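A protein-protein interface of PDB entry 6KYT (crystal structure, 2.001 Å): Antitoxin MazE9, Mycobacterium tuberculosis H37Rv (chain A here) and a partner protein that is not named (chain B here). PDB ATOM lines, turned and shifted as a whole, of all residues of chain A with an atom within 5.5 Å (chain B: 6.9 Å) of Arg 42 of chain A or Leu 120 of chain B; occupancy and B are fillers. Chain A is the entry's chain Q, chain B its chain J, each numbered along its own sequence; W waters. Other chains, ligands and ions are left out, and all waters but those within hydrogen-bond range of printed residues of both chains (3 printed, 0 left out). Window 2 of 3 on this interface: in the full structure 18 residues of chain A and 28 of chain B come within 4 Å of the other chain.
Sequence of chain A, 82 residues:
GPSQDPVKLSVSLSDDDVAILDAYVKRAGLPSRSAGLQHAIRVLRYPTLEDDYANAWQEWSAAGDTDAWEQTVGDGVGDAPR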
ATOM      1  N   LEU A  37      -3.358   7.586  20.179  1.00  0.00           N
ATOM      2  CA  LEU A  37      -4.084   8.746  19.677  1.00  0.00           C
ATOM      3  C   LEU A  37      -3.446   9.318  18.418  1.00  0.00           C
ATOM      4  O   LEU A  37      -4.142   9.929  17.602  1.00  0.00           O
ATOM      5  CB  LEU A  37      -4.185   9.815  20.762  1.00  0.00           C
ATOM      6  CG  LEU A  37      -5.196   9.480  21.860  1.00  0.00           C
ATOM      7  CD1 LEU A  37      -5.242  10.565  22.905  1.00  0.00           C
ATOM      8  CD2 LEU A  37      -6.572   9.286  21.258  1.00  0.00           C
ATOM      9  N   GLN A  38      -2.135   9.143  18.241  1.00  0.00           N
ATOM     10  CA  GLN A  38      -1.518   9.496  16.967  1.00  0.00           C
ATOM     11  C   GLN A  38      -2.090   8.640  15.843  1.00  0.00           C
ATOM     12  O   GLN A  38      -2.490   9.157  14.785  1.00  0.00           O
ATOM     13  CB  GLN A  38       0.002   9.342  17.050  1.00  0.00           C
ATOM     14  CG  GLN A  38       0.698  10.416  17.876  1.00  0.00           C
ATOM     15  CD  GLN A  38       2.210  10.347  17.767  1.00  0.00           C
ATOM     16  OE1 GLN A  38       2.791   9.264  17.695  1.00  0.00           O
ATOM     17  NE2 GLN A  38       2.855  11.508  17.743  1.00  0.00           N
ATOM     18  N   HIS A  39      -2.150   7.321  16.064  1.00  0.00           N
ATOM     19  CA  HIS A  39      -2.797   6.445  15.090  1.00  0.00           C
ATOM     20  C   HIS A  39      -4.232   6.886  14.817  1.00  0.00           C
ATOM     21  O   HIS A  39      -4.665   6.954  13.656  1.00  0.00           O
ATOM     22  CB  HIS A  39      -2.766   4.997  15.583  1.00  0.00           C
ATOM     23  CG  HIS A  39      -1.429   4.338  15.448  1.00  0.00           C
ATOM     24  ND1 HIS A  39      -1.271   3.075  14.918  1.00  0.00           N
ATOM     25  CD2 HIS A  39      -0.184   4.769  15.768  1.00  0.00           C
ATOM     26  CE1 HIS A  39       0.010   2.754  14.921  1.00  0.00           C
ATOM     27  NE2 HIS A  39       0.691   3.765  15.430  1.00  0.00           N
ATOM     28  N   ALA A  40      -4.978   7.211  15.878  1.00  0.00           N
ATOM     29  CA  ALA A  40      -6.367   7.628  15.705  1.00  0.00           C
ATOM     30  C   ALA A  40      -6.472   8.895  14.864  1.00  0.00           C
ATOM     31  O   ALA A  40      -7.360   9.010  14.010  1.00  0.00           O
ATOM     32  CB  ALA A  40      -7.022   7.838  17.068  1.00  0.00           C
ATOM     33  N   ILE A  41      -5.575   9.860  15.092  1.00  0.00           N
ATOM     34  CA  ILE A  41      -5.618  11.110  14.337  1.00  0.00           C
ATOM     35  C   ILE A  41      -5.333  10.855  12.865  1.00  0.00           C
ATOM     36  O   ILE A  41      -5.993  11.422  11.985  1.00  0.00           O
ATOM     37  CB  ILE A  41      -4.637  12.137  14.934  1.00  0.00           C
ATOM     38  CG1 ILE A  41      -5.106  12.574  16.320  1.00  0.00           C
ATOM     39  CG2 ILE A  41      -4.498  13.346  14.018  1.00  0.00           C
ATOM     40  CD1 ILE A  41      -4.039  13.272  17.125  1.00  0.00           C
ATOM     41  N   ARG A  42      -4.347  10.003  12.566  1.00  0.00           N
ATOM     42  CA  ARG A  42      -4.084   9.685  11.164  1.00  0.00           C
ATOM     43  C   ARG A  42      -5.299   9.033  10.507  1.00  0.00           C
ATOM     44  O   ARG A  42      -5.666   9.390   9.376  1.00  0.00           O
ATOM     45  CB  ARG A  42      -2.848   8.790  11.051  1.00  0.00           C
ATOM     46  CG  ARG A  42      -2.369   8.542   9.628  1.00  0.00           C
ATOM     47  CD  ARG A  42      -0.971   7.921   9.602  1.00  0.00           C
ATOM     48  NE  ARG A  42       0.085   8.886   9.911  1.00  0.00           N
ATOM     49  CZ  ARG A  42       1.385   8.599   9.916  1.00  0.00           C
ATOM     50  NH1 ARG A  42       1.795   7.372   9.625  1.00  0.00           N
ATOM     51  NH2 ARG A  42       2.278   9.539  10.202  1.00  0.00           N
ATOM     52  N   VAL A  43      -5.949   8.099  11.210  1.00  0.00           N
ATOM     53  CA  VAL A  43      -7.198   7.524  10.711  1.00  0.00           C
ATOM     54  C   VAL A  43      -8.225   8.621  10.444  1.00  0.00           C
ATOM     55  O   VAL A  43      -8.951   8.582   9.441  1.00  0.00           O
ATOM     56  CB  VAL A  43      -7.735   6.473  11.705  1.00  0.00           C
ATOM     57  CG1 VAL A  43      -9.116   6.008  11.292  1.00  0.00           C
ATOM     58  CG2 VAL A  43      -6.779   5.298  11.805  1.00  0.00           C
ATOM     59  N   LEU A  44      -8.310   9.612  11.339  1.00  0.00           N
ATOM     60  CA  LEU A  44      -9.175  10.763  11.093  1.00  0.00           C
ATOM     61  C   LEU A  44      -8.807  11.455   9.790  1.00  0.00           C
ATOM     62  O   LEU A  44      -9.687  11.870   9.026  1.00  0.00           O
ATOM     63  CB  LEU A  44      -9.088  11.760  12.248  1.00  0.00           C
ATOM     64  CG  LEU A  44     -10.189  11.797  13.305  1.00  0.00           C
ATOM     65  CD1 LEU A  44      -9.989  13.003  14.214  1.00  0.00           C
ATOM     66  CD2 LEU A  44     -11.564  11.819  12.664  1.00  0.00           C
ATOM     67  N   ARG A  45      -7.511  11.590   9.517  1.00  0.00           N
ATOM     68  CA  ARG A  45      -7.101  12.312   8.321  1.00  0.00           C
ATOM     69  C   ARG A  45      -7.424  11.544   7.044  1.00  0.00           C
ATOM     70  O   ARG A  45      -7.705  12.170   6.015  1.00  0.00           O
ATOM     71  CB  ARG A  45      -5.612  12.647   8.381  1.00  0.00           C
ATOM     72  CG  ARG A  45      -5.203  13.695   7.359  1.00  0.00           C
ATOM     73  CD  ARG A  45      -3.705  13.900   7.315  1.00  0.00           C
ATOM     74  NE  ARG A  45      -3.337  14.970   6.394  1.00  0.00           N
ATOM     75  CZ  ARG A  45      -2.099  15.425   6.240  1.00  0.00           C
ATOM     76  NH1 ARG A  45      -1.108  14.897   6.946  1.00  0.00           N
ATOM     77  NH2 ARG A  45      -1.850  16.404   5.382  1.00  0.00           N
ATOM     78  N   TYR A  46      -7.403  10.207   7.068  1.00  0.00           N
ATOM     79  CA  TYR A  46      -7.664   9.417   5.857  1.00  0.00           C
ATOM     80  C   TYR A  46      -8.826   8.456   6.088  1.00  0.00           C
ATOM     81  O   TYR A  46      -8.621   7.268   6.376  1.00  0.00           O
ATOM     82  CB  TYR A  46      -6.400   8.683   5.401  1.00  0.00           C
ATOM     83  CG  TYR A  46      -5.206   9.606   5.277  1.00  0.00           C
ATOM     84  CD1 TYR A  46      -5.122  10.543   4.252  1.00  0.00           C
ATOM     85  CD2 TYR A  46      -4.174   9.560   6.203  1.00  0.00           C
ATOM     86  CE1 TYR A  46      -4.033  11.396   4.147  1.00  0.00           C
ATOM     87  CE2 TYR A  46      -3.086  10.406   6.107  1.00  0.00           C
ATOM     88  CZ  TYR A  46      -3.018  11.322   5.079  1.00  0.00           C
ATOM     89  OH  TYR A  46      -1.933  12.164   4.989  1.00  0.00           O
ATOM     90  N   GLU B 112       5.363  12.598   3.442  1.00  0.00           N
ATOM     91  CA  GLU B 112       4.124  12.290   4.151  1.00  0.00           C
ATOM     92  C   GLU B 112       3.489  11.005   3.630  1.00  0.00           C
ATOM     93  O   GLU B 112       2.972  10.198   4.414  1.00  0.00           O
ATOM     94  CB  GLU B 112       3.145  13.457   4.037  1.00  0.00           C
ATOM     95  CG  GLU B 112       3.493  14.651   4.912  1.00  0.00           C
ATOM     96  CD  GLU B 112       3.853  14.250   6.331  1.00  0.00           C
ATOM     97  OE1 GLU B 112       4.944  14.638   6.800  1.00  0.00           O
ATOM     98  OE2 GLU B 112       3.048  13.544   6.974  1.00  0.00           O
ATOM     99  N   LEU B 114       5.043   8.451   2.259  1.00  0.00           N
ATOM    100  CA  LEU B 114       5.860   7.332   2.714  1.00  0.00           C
ATOM    101  C   LEU B 114       5.599   7.017   4.181  1.00  0.00           C
ATOM    102  O   LEU B 114       5.494   5.846   4.559  1.00  0.00           O
ATOM    103  CB  LEU B 114       7.340   7.634   2.484  1.00  0.00           C
ATOM    104  CG  LEU B 114       7.817   7.604   1.031  1.00  0.00           C
ATOM    105  CD1 LEU B 114       9.149   8.322   0.887  1.00  0.00           C
ATOM    106  CD2 LEU B 114       7.923   6.169   0.540  1.00  0.00           C
ATOM    107  N   LYS B 115       5.493   8.049   5.023  1.00  0.00           N
ATOM    108  CA  LYS B 115       5.208   7.806   6.434  1.00  0.00           C
ATOM    109  C   LYS B 115       3.820   7.200   6.618  1.00  0.00           C
ATOM    110  O   LYS B 115       3.633   6.304   7.451  1.00  0.00           O
ATOM    111  CB  LYS B 115       5.351   9.103   7.229  1.00  0.00           C
ATOM    112  CG  LYS B 115       6.800   9.520   7.447  1.00  0.00           C
ATOM    113  CD  LYS B 115       6.917  10.718   8.374  1.00  0.00           C
ATOM    114  CE  LYS B 115       6.439  11.988   7.696  1.00  0.00           C
ATOM    115  NZ  LYS B 115       6.725  13.195   8.519  1.00  0.00           N
ATOM    116  N   LEU B 116       2.839   7.667   5.840  1.00  0.00           N
ATOM    117  CA  LEU B 116       1.505   7.075   5.889  1.00  0.00           C
ATOM    118  C   LEU B 116       1.541   5.604   5.494  1.00  0.00           C
ATOM    119  O   LEU B 116       0.984   4.747   6.189  1.00  0.00           O
ATOM    120  CB  LEU B 116       0.553   7.847   4.974  1.00  0.00           C
ATOM    121  CG  LEU B 116      -0.783   7.152   4.692  1.00  0.00           C
ATOM    122  CD1 LEU B 116      -1.613   7.029   5.963  1.00  0.00           C
ATOM    123  CD2 LEU B 116      -1.561   7.871   3.598  1.00  0.00           C
ATOM    124  N   HIS B 117       2.199   5.292   4.374  1.00  0.00           N
ATOM    125  CA  HIS B 117       2.195   3.919   3.882  1.00  0.00           C
ATOM    126  C   HIS B 117       2.983   2.984   4.789  1.00  0.00           C
ATOM    127  O   HIS B 117       2.605   1.818   4.949  1.00  0.00           O
ATOM    128  CB  HIS B 117       2.756   3.862   2.462  1.00  0.00           C
ATOM    129  CG  HIS B 117       2.777   2.483   1.879  1.00  0.00           C
ATOM    130  ND1 HIS B 117       1.630   1.745   1.679  1.00  0.00           N
ATOM    131  CD2 HIS B 117       3.803   1.704   1.464  1.00  0.00           C
ATOM    132  CE1 HIS B 117       1.949   0.572   1.161  1.00  0.00           C
ATOM    133  NE2 HIS B 117       3.262   0.522   1.020  1.00  0.00           N
ATOM    134  N   LEU B 118       4.068   3.466   5.391  1.00  0.00           N
ATOM    135  CA  LEU B 118       4.953   2.627   6.187  1.00  0.00           C
ATOM    136  C   LEU B 118       4.699   2.729   7.684  1.00  0.00           C
ATOM    137  O   LEU B 118       5.459   2.147   8.464  1.00  0.00           O
ATOM    138  CB  LEU B 118       6.414   2.974   5.885  1.00  0.00           C
ATOM    139  CG  LEU B 118       6.857   2.706   4.447  1.00  0.00           C
ATOM    140  CD1 LEU B 118       8.280   3.182   4.235  1.00  0.00           C
ATOM    141  CD2 LEU B 118       6.728   1.227   4.112  1.00  0.00           C
ATOM    142  N   ASP B 119       3.659   3.455   8.101  1.00  0.00           N
ATOM    143  CA  ASP B 119       3.259   3.527   9.509  1.00  0.00           C
ATOM    144  C   ASP B 119       4.366   4.150  10.360  1.00  0.00           C
ATOM    145  O   ASP B 119       4.705   3.663  11.440  1.00  0.00           O
ATOM    146  CB  ASP B 119       2.868   2.143  10.035  1.00  0.00           C
ATOM    147  CG  ASP B 119       1.602   2.165  10.864  1.00  0.00           C
ATOM    148  OD1 ASP B 119       0.659   2.900  10.498  1.00  0.00           O
ATOM    149  OD2 ASP B 119       1.547   1.443  11.880  1.00  0.00           O
ATOM    150  N   LEU B 120       4.930   5.243   9.857  1.00  0.00           N
ATOM    151  CA  LEU B 120       6.012   5.957  10.520  1.00  0.00           C
ATOM    152  C   LEU B 120       5.537   7.339  10.949  1.00  0.00           C
ATOM    153  O   LEU B 120       4.670   7.941  10.310  1.00  0.00           O
ATOM    154  CB  LEU B 120       7.227   6.090   9.597  1.00  0.00           C
ATOM    155  CG  LEU B 120       7.790   4.789   9.022  1.00  0.00           C
ATOM    156  CD1 LEU B 120       8.912   5.079   8.036  1.00  0.00           C
ATOM    157  CD2 LEU B 120       8.272   3.875  10.137  1.00  0.00           C
ATOM    158  N   TRP B 121       6.115   7.842  12.037  1.00  0.00           N
ATOM    159  CA  TRP B 121       5.747   9.143  12.573  1.00  0.00           C
ATOM    160  C   TRP B 121       6.987   9.997  12.782  1.00  0.00           C
ATOM    161  O   TRP B 121       8.048   9.488  13.154  1.00  0.00           O
ATOM    162  CB  TRP B 121       4.968   9.004  13.888  1.00  0.00           C
ATOM    163  CG  TRP B 121       3.491   8.941  13.672  1.00  0.00           C
ATOM    164  CD1 TRP B 121       2.611   9.981  13.737  1.00  0.00           C
ATOM    165  CD2 TRP B 121       2.719   7.782  13.332  1.00  0.00           C
ATOM    166  NE1 TRP B 121       1.338   9.541  13.468  1.00  0.00           N
ATOM    167  CE2 TRP B 121       1.377   8.196  13.216  1.00  0.00           C
ATOM    168  CE3 TRP B 121       3.032   6.436  13.120  1.00  0.00           C
ATOM    169  CZ2 TRP B 121       0.349   7.311  12.897  1.00  0.00           C
ATOM    170  CZ3 TRP B 121       2.008   5.559  12.803  1.00  0.00           C
ATOM    171  CH2 TRP B 121       0.683   6.001  12.695  1.00  0.00           C
ATOM    172  N   SER B 122       6.834  11.298  12.527  1.00  0.00           N
ATOM    173  CA  SER B 122       7.894  12.303  12.659  1.00  0.00           C
ATOM    174  C   SER B 122       9.000  12.106  11.627  1.00  0.00           C
ATOM    175  O   SER B 122       9.055  12.820  10.623  1.00  0.00           O
ATOM    176  CB  SER B 122       8.484  12.290  14.073  1.00  0.00           C
ATOM    177  OG  SER B 122       7.470  12.471  15.045  1.00  0.00           O
ATOM    178  OXT SER B 122       9.862  11.239  11.764  1.00  0.00           O
HETATM  179  O   HOH W   1       0.131   5.004   8.708  1.00  0.00           O
HETATM  180  O   HOH W   2       0.826  11.584   6.391  1.00  0.00           O
HETATM  181  O   HOH W   3      -1.096  11.259  13.531  1.00  0.00           O
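The guanidinium group (NH2) of Arg 42 of chain A sits close to the indole nitrogen (NE1) of Trp 121 of chain B, at 3.4 Å.
The backbone carbonyl oxygen (O) of Leu 120 of chain B is in hydrogen-bond range of the guanidinium group (NH2) of Arg 42 of chain A (2.9 Å).
The backbone carbonyl oxygen of Lys 115 of chain B sits at hydrogen-bond distance from the guanidinium group of Arg 42 of chain A.
The chain-end carboxylate (O) of Ser 122 of chain B lies within salt-bridge range of the side-chain amino group (NZ) of Lys 115 of chain B (3.2 Å).
The backbone carbonyl oxygen (O) of Lys 115 of chain B sits at hydrogen-bond distance from the backbone NH (N) of Leu 120 of chain B, 2.9 Å away.
The side-chain carboxylate (OE1) of Glu 112 of chain B is in salt-bridge range of the side-chain amino group (NZ) of Lys 115 of chain B, 2.9 Å away.
The guanidinium group of Arg 45 of chain A lies close to the side-chain hydroxyl of Tyr 46 of chain A (3.4 Å).
Trp 121 of chain B touches Gln 38 of chain A.
His 39 of chain A touches Asp 119 of chain B (CE1 to OD2, 3.7 Å).
His 39 of chain A touches Trp 121 of chain B.
Leu 116 of chain B touches Arg 42 of chain A (CA to NH1, 3.8 Å).
CD1 of Leu 116 of chain B touches CD2 of Tyr 46 of chain A, 3.6 Å away.
Of chain B, only Lys 115, Leu 116, Leu 120 and Trp 121 come within 4 Å of Arg 42 of chain A.
Leu 120 of chain B touches one residue of chain A.
Of the printed residues of chain A, Lys 115 of chain B touches Arg 42 (3.0 Å).
Of the printed residues of chain B, Gln 38 of chain A touches Trp 121 (3.8 Å).
Of the printed residues of chain A, Leu 116 of chain B touches Arg 42 (3.8 Å) and Tyr 46 (3.6 Å).
Of the printed residues of chain A, Asp 119 of chain B touches His 39 (3.7 Å).
Printed residues of chain B within 4 Å of Tyr 46 of chain A: Leu 116 (3.6 Å).
His 117 of chain B touches none of the printed residues of chain A.
Ser 122 of chain B touches none of the printed residues of chain A.
The nearest printed residue of chain A that does not touch Leu 120 of chain B is His 39 of chain A (7.2 Å).
Printed residues of chain A that touch a printed residue of chain B: Gln 38, His 39, Arg 42 and Tyr 46.
Hydrophobic or aromatic side chains of chain A within 4 Å of the printed part of chain B: His 39 and Tyr 46.
Among the printed residues, 8 pairs touch across the chains.
Among the printed residues, no Asp or Glu carboxylate lies within 4 Å of a Lys or Arg side-chain nitrogen of the other chain.
Water W1 lies within hydrogen-bond range of O of Leu 116 of chain B (2.7 Å), OD1 of Asp 119 of chain B (2.8 Å) and NH1 of Arg 42 of chain A (3.0 Å).
Water W3 lies within hydrogen-bond range of O of Gln 38 of chain A (2.8 Å) and NE1 of Trp 121 of chain B (3.0 Å).
Water W2 lies within hydrogen-bond range of OE2 of Glu 112 of chain B (3.0 Å) and OH of Tyr 46 of chain A (3.1 Å).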
